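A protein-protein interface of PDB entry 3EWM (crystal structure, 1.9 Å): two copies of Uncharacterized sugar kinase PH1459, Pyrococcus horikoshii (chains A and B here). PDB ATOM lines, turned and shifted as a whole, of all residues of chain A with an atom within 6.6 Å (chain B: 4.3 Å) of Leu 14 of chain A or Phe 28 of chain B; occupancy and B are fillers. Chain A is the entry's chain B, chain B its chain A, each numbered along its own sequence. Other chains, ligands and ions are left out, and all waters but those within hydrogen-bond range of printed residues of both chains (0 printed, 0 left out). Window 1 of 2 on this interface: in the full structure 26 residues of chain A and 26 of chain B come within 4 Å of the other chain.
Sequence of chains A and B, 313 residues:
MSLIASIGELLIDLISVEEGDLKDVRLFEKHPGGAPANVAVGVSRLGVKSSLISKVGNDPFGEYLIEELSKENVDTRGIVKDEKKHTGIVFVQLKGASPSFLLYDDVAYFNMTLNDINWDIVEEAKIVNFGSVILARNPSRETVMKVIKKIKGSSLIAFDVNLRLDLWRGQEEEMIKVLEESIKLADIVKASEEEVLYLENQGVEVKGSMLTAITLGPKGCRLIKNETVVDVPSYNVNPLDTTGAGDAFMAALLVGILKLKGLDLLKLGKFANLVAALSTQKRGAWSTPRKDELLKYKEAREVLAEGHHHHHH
Leu 14 of chain A touches Phe 28 of chain B, and with the chains exchanged Phe 28 of chain A touches Leu 14 of chain B. Phe 28 of chain A touches Lys 30 of chain B, and with the chains exchanged Lys 30 of chain A touches Phe 28 of chain B. Glu 29 of chain A touches Leu 27 of chain B, but with the chains exchanged Leu 27 of chain A does not touch Glu 29 of chain B (4.05 Å). Phe 91 of chain B touches its own counterpart, Phe 91 of chain A. Positions printed for both chains: 14, 15, 16, 22, 27, 28, 29, 30 and 91. Of the 20 pairs that touch across the chains among the printed residues, 12 have their exchanged pair printed and touching as well.
The backbone carbonyl oxygen (O) of Phe 28 of chain B lies within hydrogen-bond range of the backbone NH (N) of Phe 28 of chain A (2.9 Å). The backbone carbonyl oxygen (O) of Val 25 of chain B is in hydrogen-bond range of the side-chain amino group (NZ) of Lys 30 of chain A. N of Lys 30 of chain B lies within hydrogen-bond range of O of Arg 26 of chain A.
O of Ile 15 of chain A is in hydrogen-bond range of N of Glu 29 of chain A. The backbone carbonyl oxygen (O) of Leu 14 of chain A is in hydrogen-bond range of the backbone NH (N) of Val 92 of chain A, at 2.8 Å. A ring nitrogen (NE2) of His 31 of chain A sits at hydrogen-bond distance from the side-chain carboxylate (OE1) of Glu 29 of chain A. The backbone NH of Ile 15 of chain B is in hydrogen-bond range of the backbone carbonyl oxygen of Glu 29 of chain B, 2.7 Å away. N of Leu 14 of chain A is in hydrogen-bond range of O of Val 90 of chain A.
Of chain B, only Phe 28 and Phe 91 come within 4 Å of Leu 14 of chain A. Of the printed residues of chain B, Lys 30 of chain A touches Leu 22 (3.8 Å), Val 25 (2.6 Å) and Phe 28 (3.96 Å). Ile 15 of chain B touches none of the printed residues of chain A. Of the printed residues of chain A, Val 25 of chain B touches Lys 30. Of the printed residues of chain A, Leu 27 of chain B touches Phe 28 and Glu 29. Of chain A, only Leu 14 (3.9 Å), Arg 26 (3.9 Å), Leu 27 (3.5 Å), Phe 28 (2.9 Å), Lys 30 (3.96 Å) and Phe 61 (3.9 Å) come within 4 Å of Phe 28 of chain B. The nearest residue of chain A that does not touch Phe 28 of chain B is Glu 29 of chain A (5.1 Å).
Printed residues of chain B that touch a printed residue of chain A: Leu 14, Leu 22, Val 25, Leu 27, Phe 28, Glu 29, Lys 30 and Phe 91.
Among the printed residues, merely in contact across the chains: Leu 14 of chain A with Phe 28 of chain B (3.9 Å), Leu 14 of chain A with Phe 91 of chain B (3.6 Å), Leu 22 of chain A with Lys 30 of chain B (3.6 Å), Arg 26 of chain A with Phe 28 of chain B (3.9 Å), Arg 26 of chain A with Glu 29 of chain B (3.2 Å), Leu 27 of chain A with Phe 28 of chain B (3.5 Å), Phe 28 of chain A with Leu 14 of chain B (3.8 Å), Phe 28 of chain A with Leu 27 of chain B (3.4 Å), Phe 28 of chain A with Lys 30 of chain B (3.9 Å), Glu 29 of chain A with Leu 27 of chain B (3.7 Å), Lys 30 of chain A with Leu 22 of chain B (3.8 Å), Lys 30 of chain A with Phe 28 of chain B (3.96 Å), Phe 61 of chain A with Leu 22 of chain B (3.5 Å), Phe 61 of chain A with Phe 28 of chain B (3.9 Å), Phe 61 of chain A with Phe 91 of chain B (3.5 Å), Phe 91 of chain A with Leu 14 of chain B (3.5 Å) and Phe 91 of chain A with Phe 91 of chain B (3.96 Å).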
ATOM      1  N   LEU A  11     -14.987  -3.181  13.501  1.00  0.00           N
ATOM      2  CA  LEU A  11     -13.940  -3.374  12.536  1.00  0.00           C
ATOM      3  C   LEU A  11     -13.418  -4.794  12.582  1.00  0.00           C
ATOM      4  O   LEU A  11     -13.738  -5.560  13.504  1.00  0.00           O
ATOM      5  CB  LEU A  11     -12.819  -2.344  12.773  1.00  0.00           C
ATOM      6  CG  LEU A  11     -12.165  -2.251  14.168  1.00  0.00           C
ATOM      7  CD1 LEU A  11     -11.361  -3.489  14.527  1.00  0.00           C
ATOM      8  CD2 LEU A  11     -11.266  -1.064  14.149  1.00  0.00           C
ATOM      9  N   ILE A  12     -12.642  -5.145  11.565  1.00  0.00           N
ATOM     10  CA  ILE A  12     -11.923  -6.421  11.548  1.00  0.00           C
ATOM     11  C   ILE A  12     -10.559  -6.249  12.185  1.00  0.00           C
ATOM     12  O   ILE A  12      -9.756  -5.442  11.724  1.00  0.00           O
ATOM     13  CB  ILE A  12     -11.681  -6.912  10.110  1.00  0.00           C
ATOM     14  CG1 ILE A  12     -12.987  -6.918   9.313  1.00  0.00           C
ATOM     15  CG2 ILE A  12     -10.941  -8.286  10.124  1.00  0.00           C
ATOM     16  CD1 ILE A  12     -13.880  -8.127   9.602  1.00  0.00           C
ATOM     17  N   ASP A  13     -10.288  -7.036  13.217  1.00  0.00           N
ATOM     18  CA  ASP A  13      -8.933  -7.143  13.760  1.00  0.00           C
ATOM     19  C   ASP A  13      -8.240  -8.245  12.986  1.00  0.00           C
ATOM     20  O   ASP A  13      -8.684  -9.391  13.011  1.00  0.00           O
ATOM     21  CB  ASP A  13      -8.968  -7.545  15.228  1.00  0.00           C
ATOM     22  CG  ASP A  13      -9.205  -6.373  16.149  1.00  0.00           C
ATOM     23  OD1 ASP A  13      -8.991  -5.236  15.710  1.00  0.00           O
ATOM     24  OD2 ASP A  13      -9.586  -6.592  17.310  1.00  0.00           O
ATOM     25  N   LEU A  14      -7.181  -7.880  12.279  1.00  0.00           N
ATOM     26  CA  LEU A  14      -6.300  -8.859  11.644  1.00  0.00           C
ATOM     27  C   LEU A  14      -5.153  -9.061  12.599  1.00  0.00           C
ATOM     28  O   LEU A  14      -4.227  -8.267  12.688  1.00  0.00           O
ATOM     29  CB  LEU A  14      -5.860  -8.375  10.264  1.00  0.00           C
ATOM     30  CG  LEU A  14      -7.179  -8.476   9.484  1.00  0.00           C
ATOM     31  CD1 LEU A  14      -7.513  -7.208   8.704  1.00  0.00           C
ATOM     32  CD2 LEU A  14      -7.240  -9.753   8.652  1.00  0.00           C
ATOM     33  N   ILE A  15      -5.278 -10.111  13.380  1.00  0.00           N
ATOM     34  CA  ILE A  15      -4.352 -10.306  14.453  1.00  0.00           C
ATOM     35  C   ILE A  15      -3.182 -11.164  13.994  1.00  0.00           C
ATOM     36  O   ILE A  15      -3.373 -12.264  13.485  1.00  0.00           O
ATOM     37  CB  ILE A  15      -5.049 -10.931  15.662  1.00  0.00           C
ATOM     38  CG1 ILE A  15      -6.285 -10.079  16.020  1.00  0.00           C
ATOM     39  CG2 ILE A  15      -4.047 -11.014  16.819  1.00  0.00           C
ATOM     40  CD1 ILE A  15      -7.071 -10.542  17.214  1.00  0.00           C
ATOM     41  N   SER A  16      -1.982 -10.630  14.174  1.00  0.00           N
ATOM     42  CA  SER A  16      -0.733 -11.315  13.859  1.00  0.00           C
ATOM     43  C   SER A  16      -0.669 -12.626  14.614  1.00  0.00           C
ATOM     44  O   SER A  16      -0.765 -12.646  15.845  1.00  0.00           O
ATOM     45  CB  SER A  16       0.464 -10.472  14.275  1.00  0.00           C
ATOM     46  OG  SER A  16       0.545  -9.256  13.549  1.00  0.00           O
ATOM     47  N   LEU A  22       4.879  -5.649  12.535  1.00  0.00           N
ATOM     48  CA  LEU A  22       3.894  -5.820  11.474  1.00  0.00           C
ATOM     49  C   LEU A  22       4.520  -5.931  10.095  1.00  0.00           C
ATOM     50  O   LEU A  22       4.010  -6.659   9.243  1.00  0.00           O
ATOM     51  CB  LEU A  22       2.875  -4.677  11.514  1.00  0.00           C
ATOM     52  CG  LEU A  22       1.927  -4.751  12.708  1.00  0.00           C
ATOM     53  CD1 LEU A  22       1.207  -3.410  12.916  1.00  0.00           C
ATOM     54  CD2 LEU A  22       0.930  -5.936  12.560  1.00  0.00           C
ATOM     55  N   ARG A  26       3.710 -12.520   8.765  1.00  0.00           N
ATOM     56  CA  ARG A  26       3.352 -13.192   7.525  1.00  0.00           C
ATOM     57  C   ARG A  26       1.925 -13.728   7.536  1.00  0.00           C
ATOM     58  O   ARG A  26       1.351 -14.023   6.474  1.00  0.00           O
ATOM     59  CB  ARG A  26       4.324 -14.356   7.305  1.00  0.00           C
ATOM     60  CG  ARG A  26       5.747 -13.920   7.036  1.00  0.00           C
ATOM     61  CD  ARG A  26       6.754 -15.081   7.136  1.00  0.00           C
ATOM     62  NE  ARG A  26       7.099 -15.388   8.528  1.00  0.00           N
ATOM     63  CZ  ARG A  26       8.155 -16.102   8.910  1.00  0.00           C
ATOM     64  NH1 ARG A  26       9.002 -16.582   8.010  1.00  0.00           N
ATOM     65  NH2 ARG A  26       8.371 -16.320  10.203  1.00  0.00           N
ATOM     66  N   LEU A  27       1.371 -13.898   8.734  1.00  0.00           N
ATOM     67  CA  LEU A  27       0.069 -14.522   8.908  1.00  0.00           C
ATOM     68  C   LEU A  27      -0.806 -13.765   9.898  1.00  0.00           C
ATOM     69  O   LEU A  27      -0.408 -13.536  11.050  1.00  0.00           O
ATOM     70  CB  LEU A  27       0.228 -15.973   9.364  1.00  0.00           C
ATOM     71  CG  LEU A  27      -1.035 -16.848   9.433  1.00  0.00           C
ATOM     72  CD1 LEU A  27      -1.770 -16.975   8.083  1.00  0.00           C
ATOM     73  CD2 LEU A  27      -0.709 -18.234   9.986  1.00  0.00           C
ATOM     74  N   PHE A  28      -2.015 -13.436   9.446  1.00  0.00           N
ATOM     75  CA  PHE A  28      -3.013 -12.755  10.257  1.00  0.00           C
ATOM     76  C   PHE A  28      -4.287 -13.577  10.409  1.00  0.00           C
ATOM     77  O   PHE A  28      -4.764 -14.202   9.450  1.00  0.00           O
ATOM     78  CB  PHE A  28      -3.377 -11.414   9.634  1.00  0.00           C
ATOM     79  CG  PHE A  28      -2.237 -10.440   9.593  1.00  0.00           C
ATOM     80  CD1 PHE A  28      -1.983  -9.604  10.668  1.00  0.00           C
ATOM     81  CD2 PHE A  28      -1.391 -10.399   8.497  1.00  0.00           C
ATOM     82  CE1 PHE A  28      -0.939  -8.709  10.642  1.00  0.00           C
ATOM     83  CE2 PHE A  28      -0.326  -9.501   8.462  1.00  0.00           C
ATOM     84  CZ  PHE A  28      -0.102  -8.656   9.546  1.00  0.00           C
ATOM     85  N   GLU A  29      -4.840 -13.569  11.617  1.00  0.00           N
ATOM     86  CA  GLU A  29      -6.128 -14.190  11.850  1.00  0.00           C
ATOM     87  C   GLU A  29      -7.184 -13.120  11.999  1.00  0.00           C
ATOM     88  O   GLU A  29      -7.017 -12.173  12.758  1.00  0.00           O
ATOM     89  CB  GLU A  29      -6.082 -15.069  13.092  1.00  0.00           C
ATOM     90  CG  GLU A  29      -7.267 -15.966  13.251  1.00  0.00           C
ATOM     91  CD  GLU A  29      -7.042 -16.944  14.390  1.00  0.00           C
ATOM     92  OE1 GLU A  29      -6.958 -16.496  15.546  1.00  0.00           O
ATOM     93  OE2 GLU A  29      -6.893 -18.144  14.115  1.00  0.00           O
ATOM     94  N   LYS A  30      -8.258 -13.278  11.244  1.00  0.00           N
ATOM     95  CA  LYS A  30      -9.381 -12.355  11.259  1.00  0.00           C
ATOM     96  C   LYS A  30     -10.320 -12.580  12.456  1.00  0.00           C
ATOM     97  O   LYS A  30     -10.790 -13.706  12.717  1.00  0.00           O
ATOM     98  CB  LYS A  30     -10.112 -12.451   9.918  1.00  0.00           C
ATOM     99  CG  LYS A  30     -11.568 -12.079   9.888  1.00  0.00           C
ATOM    100  CD  LYS A  30     -12.035 -11.928   8.451  1.00  0.00           C
ATOM    101  CE  LYS A  30     -13.464 -12.434   8.281  1.00  0.00           C
ATOM    102  NZ  LYS A  30     -13.527 -13.916   8.376  1.00  0.00           N
ATOM    103  N   HIS A  31     -10.595 -11.485  13.159  1.00  0.00           N
ATOM    104  CA  HIS A  31     -11.491 -11.479  14.312  1.00  0.00           C
ATOM    105  C   HIS A  31     -12.323 -10.209  14.298  1.00  0.00           C
ATOM    106  O   HIS A  31     -11.869  -9.180  13.787  1.00  0.00           O
ATOM    107  CB  HIS A  31     -10.687 -11.529  15.602  1.00  0.00           C
ATOM    108  CG  HIS A  31      -9.929 -12.798  15.773  1.00  0.00           C
ATOM    109  ND1 HIS A  31     -10.549 -13.997  16.052  1.00  0.00           N
ATOM    110  CD2 HIS A  31      -8.609 -13.069  15.669  1.00  0.00           C
ATOM    111  CE1 HIS A  31      -9.638 -14.952  16.128  1.00  0.00           C
ATOM    112  NE2 HIS A  31      -8.452 -14.414  15.907  1.00  0.00           N
ATOM    113  N   PHE A  61     -16.560  -8.284   4.744  1.00  0.00           N
ATOM    114  CA  PHE A  61     -16.104  -8.018   6.107  1.00  0.00           C
ATOM    115  C   PHE A  61     -17.185  -7.366   6.973  1.00  0.00           C
ATOM    116  O   PHE A  61     -17.306  -7.666   8.179  1.00  0.00           O
ATOM    117  CB  PHE A  61     -14.803  -7.211   6.099  1.00  0.00           C
ATOM    118  CG  PHE A  61     -13.591  -8.025   5.720  1.00  0.00           C
ATOM    119  CD1 PHE A  61     -13.700  -9.400   5.479  1.00  0.00           C
ATOM    120  CD2 PHE A  61     -12.335  -7.431   5.652  1.00  0.00           C
ATOM    121  CE1 PHE A  61     -12.577 -10.168   5.137  1.00  0.00           C
ATOM    122  CE2 PHE A  61     -11.212  -8.179   5.330  1.00  0.00           C
ATOM    123  CZ  PHE A  61     -11.331  -9.556   5.064  1.00  0.00           C
ATOM    124  N   GLY A  88     -13.980  -1.192   8.421  1.00  0.00           N
ATOM    125  CA  GLY A  88     -12.797  -0.906   9.207  1.00  0.00           C
ATOM    126  C   GLY A  88     -11.904  -2.131   9.332  1.00  0.00           C
ATOM    127  O   GLY A  88     -12.379  -3.258   9.498  1.00  0.00           O
ATOM    128  N   ILE A  89     -10.607  -1.906   9.213  1.00  0.00           N
ATOM    129  CA  ILE A  89      -9.629  -2.932   9.431  1.00  0.00           C
ATOM    130  C   ILE A  89      -8.493  -2.349  10.268  1.00  0.00           C
ATOM    131  O   ILE A  89      -8.152  -1.162  10.176  1.00  0.00           O
ATOM    132  CB  ILE A  89      -9.062  -3.499   8.092  1.00  0.00           C
ATOM    133  CG1 ILE A  89      -8.535  -2.357   7.231  1.00  0.00           C
ATOM    134  CG2 ILE A  89     -10.133  -4.343   7.335  1.00  0.00           C
ATOM    135  CD1 ILE A  89      -7.641  -2.771   6.146  1.00  0.00           C
ATOM    136  N   VAL A  90      -7.943  -3.196  11.115  1.00  0.00           N
ATOM    137  CA  VAL A  90      -6.733  -2.875  11.819  1.00  0.00           C
ATOM    138  C   VAL A  90      -5.876  -4.137  11.882  1.00  0.00           C
ATOM    139  O   VAL A  90      -6.362  -5.238  12.189  1.00  0.00           O
ATOM    140  CB  VAL A  90      -7.016  -2.293  13.237  1.00  0.00           C
ATOM    141  CG1 VAL A  90      -8.029  -3.124  13.963  1.00  0.00           C
ATOM    142  CG2 VAL A  90      -5.735  -2.159  14.057  1.00  0.00           C
ATOM    143  N   PHE A  91      -4.610  -3.963  11.578  1.00  0.00           N
ATOM    144  CA  PHE A  91      -3.633  -5.048  11.692  1.00  0.00           C
ATOM    145  C   PHE A  91      -2.977  -4.901  13.027  1.00  0.00           C
ATOM    146  O   PHE A  91      -2.453  -3.837  13.341  1.00  0.00           O
ATOM    147  CB  PHE A  91      -2.620  -4.954  10.580  1.00  0.00           C
ATOM    148  CG  PHE A  91      -3.226  -5.110   9.237  1.00  0.00           C
ATOM    149  CD1 PHE A  91      -3.319  -6.373   8.648  1.00  0.00           C
ATOM    150  CD2 PHE A  91      -3.777  -4.005   8.585  1.00  0.00           C
ATOM    151  CE1 PHE A  91      -3.914  -6.534   7.401  1.00  0.00           C
ATOM    152  CE2 PHE A  91      -4.388  -4.157   7.352  1.00  0.00           C
ATOM    153  CZ  PHE A  91      -4.449  -5.427   6.756  1.00  0.00           C
ATOM    154  N   VAL A  92      -3.052  -5.967  13.814  1.00  0.00           N
ATOM    155  CA  VAL A  92      -2.712  -5.918  15.224  1.00  0.00           C
ATOM    156  C   VAL A  92      -1.547  -6.851  15.524  1.00  0.00           C
ATOM    157  O   VAL A  92      -1.554  -8.020  15.134  1.00  0.00           O
ATOM    158  CB  VAL A  92      -3.942  -6.297  16.094  1.00  0.00           C
ATOM    159  CG1 VAL A  92      -3.607  -6.234  17.576  1.00  0.00           C
ATOM    160  CG2 VAL A  92      -5.140  -5.389  15.794  1.00  0.00           C
ATOM    161  N   GLN A  93      -0.530  -6.321  16.195  1.00  0.00           N
ATOM    162  CA  GLN A  93       0.475  -7.176  16.788  1.00  0.00           C
ATOM    163  C   GLN A  93       0.364  -7.042  18.289  1.00  0.00           C
ATOM    164  O   GLN A  93       0.795  -6.037  18.857  1.00  0.00           O
ATOM    165  CB  GLN A  93       1.876  -6.809  16.327  1.00  0.00           C
ATOM    166  CG  GLN A  93       2.981  -7.624  17.021  1.00  0.00           C
ATOM    167  CD  GLN A  93       2.756  -9.115  16.900  1.00  0.00           C
ATOM    168  OE1 GLN A  93       2.057  -9.711  17.708  1.00  0.00           O
ATOM    169  NE2 GLN A  93       3.358  -9.725  15.891  1.00  0.00           N
ATOM    170  N   LEU B  14      -3.428  -9.888   1.006  1.00  0.00           N
ATOM    171  CA  LEU B  14      -3.715 -10.733   2.155  1.00  0.00           C
ATOM    172  C   LEU B  14      -4.452 -11.929   1.606  1.00  0.00           C
ATOM    173  O   LEU B  14      -5.604 -11.846   1.208  1.00  0.00           O
ATOM    174  CB  LEU B  14      -4.503  -9.970   3.199  1.00  0.00           C
ATOM    175  CG  LEU B  14      -3.509  -8.982   3.821  1.00  0.00           C
ATOM    176  CD1 LEU B  14      -4.134  -7.597   3.995  1.00  0.00           C
ATOM    177  CD2 LEU B  14      -2.936  -9.540   5.099  1.00  0.00           C
ATOM    178  N   ILE B  15      -3.733 -13.036   1.504  1.00  0.00           N
ATOM    179  CA  ILE B  15      -4.251 -14.164   0.745  1.00  0.00           C
ATOM    180  C   ILE B  15      -4.835 -15.206   1.665  1.00  0.00           C
ATOM    181  O   ILE B  15      -4.125 -15.770   2.499  1.00  0.00           O
ATOM    182  CB  ILE B  15      -3.163 -14.792  -0.125  1.00  0.00           C
ATOM    183  CG1 ILE B  15      -2.543 -13.688  -0.996  1.00  0.00           C
ATOM    184  CG2 ILE B  15      -3.749 -15.904  -0.993  1.00  0.00           C
ATOM    185  CD1 ILE B  15      -1.742 -14.166  -2.100  1.00  0.00           C
ATOM    186  N   SER B  16      -6.126 -15.452   1.478  1.00  0.00           N
ATOM    187  CA  SER B  16      -6.837 -16.516   2.179  1.00  0.00           C
ATOM    188  C   SER B  16      -6.007 -17.788   2.130  1.00  0.00           C
ATOM    189  O   SER B  16      -5.536 -18.215   1.071  1.00  0.00           O
ATOM    190  CB  SER B  16      -8.195 -16.783   1.552  1.00  0.00           C
ATOM    191  OG  SER B  16      -9.004 -15.610   1.491  1.00  0.00           O
ATOM    192  N   LEU B  22     -14.599 -14.778   1.441  1.00  0.00           N
ATOM    193  CA  LEU B  22     -13.831 -13.848   2.276  1.00  0.00           C
ATOM    194  C   LEU B  22     -14.501 -13.553   3.603  1.00  0.00           C
ATOM    195  O   LEU B  22     -13.824 -13.355   4.613  1.00  0.00           O
ATOM    196  CB  LEU B  22     -13.620 -12.509   1.558  1.00  0.00           C
ATOM    197  CG  LEU B  22     -12.592 -12.508   0.440  1.00  0.00           C
ATOM    198  CD1 LEU B  22     -12.666 -11.165  -0.283  1.00  0.00           C
ATOM    199  CD2 LEU B  22     -11.208 -12.778   1.030  1.00  0.00           C
ATOM    200  N   VAL B  25     -13.343 -16.645   5.624  1.00  0.00           N
ATOM    201  CA  VAL B  25     -11.920 -16.954   5.708  1.00  0.00           C
ATOM    202  C   VAL B  25     -11.322 -16.407   7.012  1.00  0.00           C
ATOM    203  O   VAL B  25     -11.520 -15.255   7.358  1.00  0.00           O
ATOM    204  CB  VAL B  25     -11.131 -16.449   4.489  1.00  0.00           C
ATOM    205  CG1 VAL B  25      -9.610 -16.599   4.746  1.00  0.00           C
ATOM    206  CG2 VAL B  25     -11.517 -17.246   3.249  1.00  0.00           C
ATOM    207  N   LEU B  27      -7.916 -16.921   8.001  1.00  0.00           N
ATOM    208  CA  LEU B  27      -6.475 -16.712   7.983  1.00  0.00           C
ATOM    209  C   LEU B  27      -6.011 -16.145   6.658  1.00  0.00           C
ATOM    210  O   LEU B  27      -6.375 -16.639   5.603  1.00  0.00           O
ATOM    211  CB  LEU B  27      -5.721 -18.032   8.201  1.00  0.00           C
ATOM    212  CG  LEU B  27      -5.309 -18.671   9.538  1.00  0.00           C
ATOM    213  CD1 LEU B  27      -5.007 -17.714  10.681  1.00  0.00           C
ATOM    214  CD2 LEU B  27      -6.256 -19.790   9.957  1.00  0.00           C
ATOM    215  N   PHE B  28      -5.161 -15.136   6.737  1.00  0.00           N
ATOM    216  CA  PHE B  28      -4.606 -14.487   5.567  1.00  0.00           C
ATOM    217  C   PHE B  28      -3.104 -14.407   5.671  1.00  0.00           C
ATOM    218  O   PHE B  28      -2.568 -13.877   6.654  1.00  0.00           O
ATOM    219  CB  PHE B  28      -5.151 -13.076   5.431  1.00  0.00           C
ATOM    220  CG  PHE B  28      -6.620 -13.024   5.252  1.00  0.00           C
ATOM    221  CD1 PHE B  28      -7.179 -13.167   3.990  1.00  0.00           C
ATOM    222  CD2 PHE B  28      -7.461 -12.859   6.353  1.00  0.00           C
ATOM    223  CE1 PHE B  28      -8.557 -13.108   3.817  1.00  0.00           C
ATOM    224  CE2 PHE B  28      -8.841 -12.810   6.186  1.00  0.00           C
ATOM    225  CZ  PHE B  28      -9.389 -12.934   4.925  1.00  0.00           C
ATOM    226  N   GLU B  29      -2.442 -14.946   4.647  1.00  0.00           N
ATOM    227  CA  GLU B  29      -1.022 -14.765   4.437  1.00  0.00           C
ATOM    228  C   GLU B  29      -0.717 -13.428   3.755  1.00  0.00           C
ATOM    229  O   GLU B  29      -1.332 -13.080   2.738  1.00  0.00           O
ATOM    230  CB  GLU B  29      -0.504 -15.887   3.554  1.00  0.00           C
ATOM    231  CG  GLU B  29       0.458 -16.804   4.229  1.00  0.00           C
ATOM    232  CD  GLU B  29       1.286 -17.573   3.233  1.00  0.00           C
ATOM    233  OE1 GLU B  29       0.694 -18.153   2.315  1.00  0.00           O
ATOM    234  OE2 GLU B  29       2.534 -17.564   3.351  1.00  0.00           O
ATOM    235  N   LYS B  30       0.261 -12.712   4.299  1.00  0.00           N
ATOM    236  CA  LYS B  30       0.659 -11.411   3.781  1.00  0.00           C
ATOM    237  C   LYS B  30       1.751 -11.601   2.733  1.00  0.00           C
ATOM    238  O   LYS B  30       2.772 -12.248   2.981  1.00  0.00           O
ATOM    239  CB  LYS B  30       1.135 -10.501   4.926  1.00  0.00           C
ATOM    240  CG  LYS B  30       2.039  -9.326   4.526  1.00  0.00           C
ATOM    241  CD  LYS B  30       2.165  -8.316   5.692  1.00  0.00           C
ATOM    242  CE  LYS B  30       3.604  -7.810   5.853  1.00  0.00           C
ATOM    243  NZ  LYS B  30       4.570  -8.917   6.236  1.00  0.00           N
ATOM    244  N   PHE B  91      -7.640  -8.063   0.196  1.00  0.00           N
ATOM    245  CA  PHE B  91      -7.929  -9.387   0.732  1.00  0.00           C
ATOM    246  C   PHE B  91      -8.382 -10.236  -0.429  1.00  0.00           C
ATOM    247  O   PHE B  91      -9.240  -9.822  -1.196  1.00  0.00           O
ATOM    248  CB  PHE B  91      -9.007  -9.293   1.802  1.00  0.00           C
ATOM    249  CG  PHE B  91      -8.585  -8.471   2.986  1.00  0.00           C
ATOM    250  CD1 PHE B  91      -7.961  -9.080   4.086  1.00  0.00           C
ATOM    251  CD2 PHE B  91      -8.769  -7.086   2.992  1.00  0.00           C
ATOM    252  CE1 PHE B  91      -7.544  -8.329   5.165  1.00  0.00           C
ATOM    253  CE2 PHE B  91      -8.351  -6.327   4.080  1.00  0.00           C
ATOM    254  CZ  PHE B  91      -7.733  -6.955   5.161  1.00  0.00           C
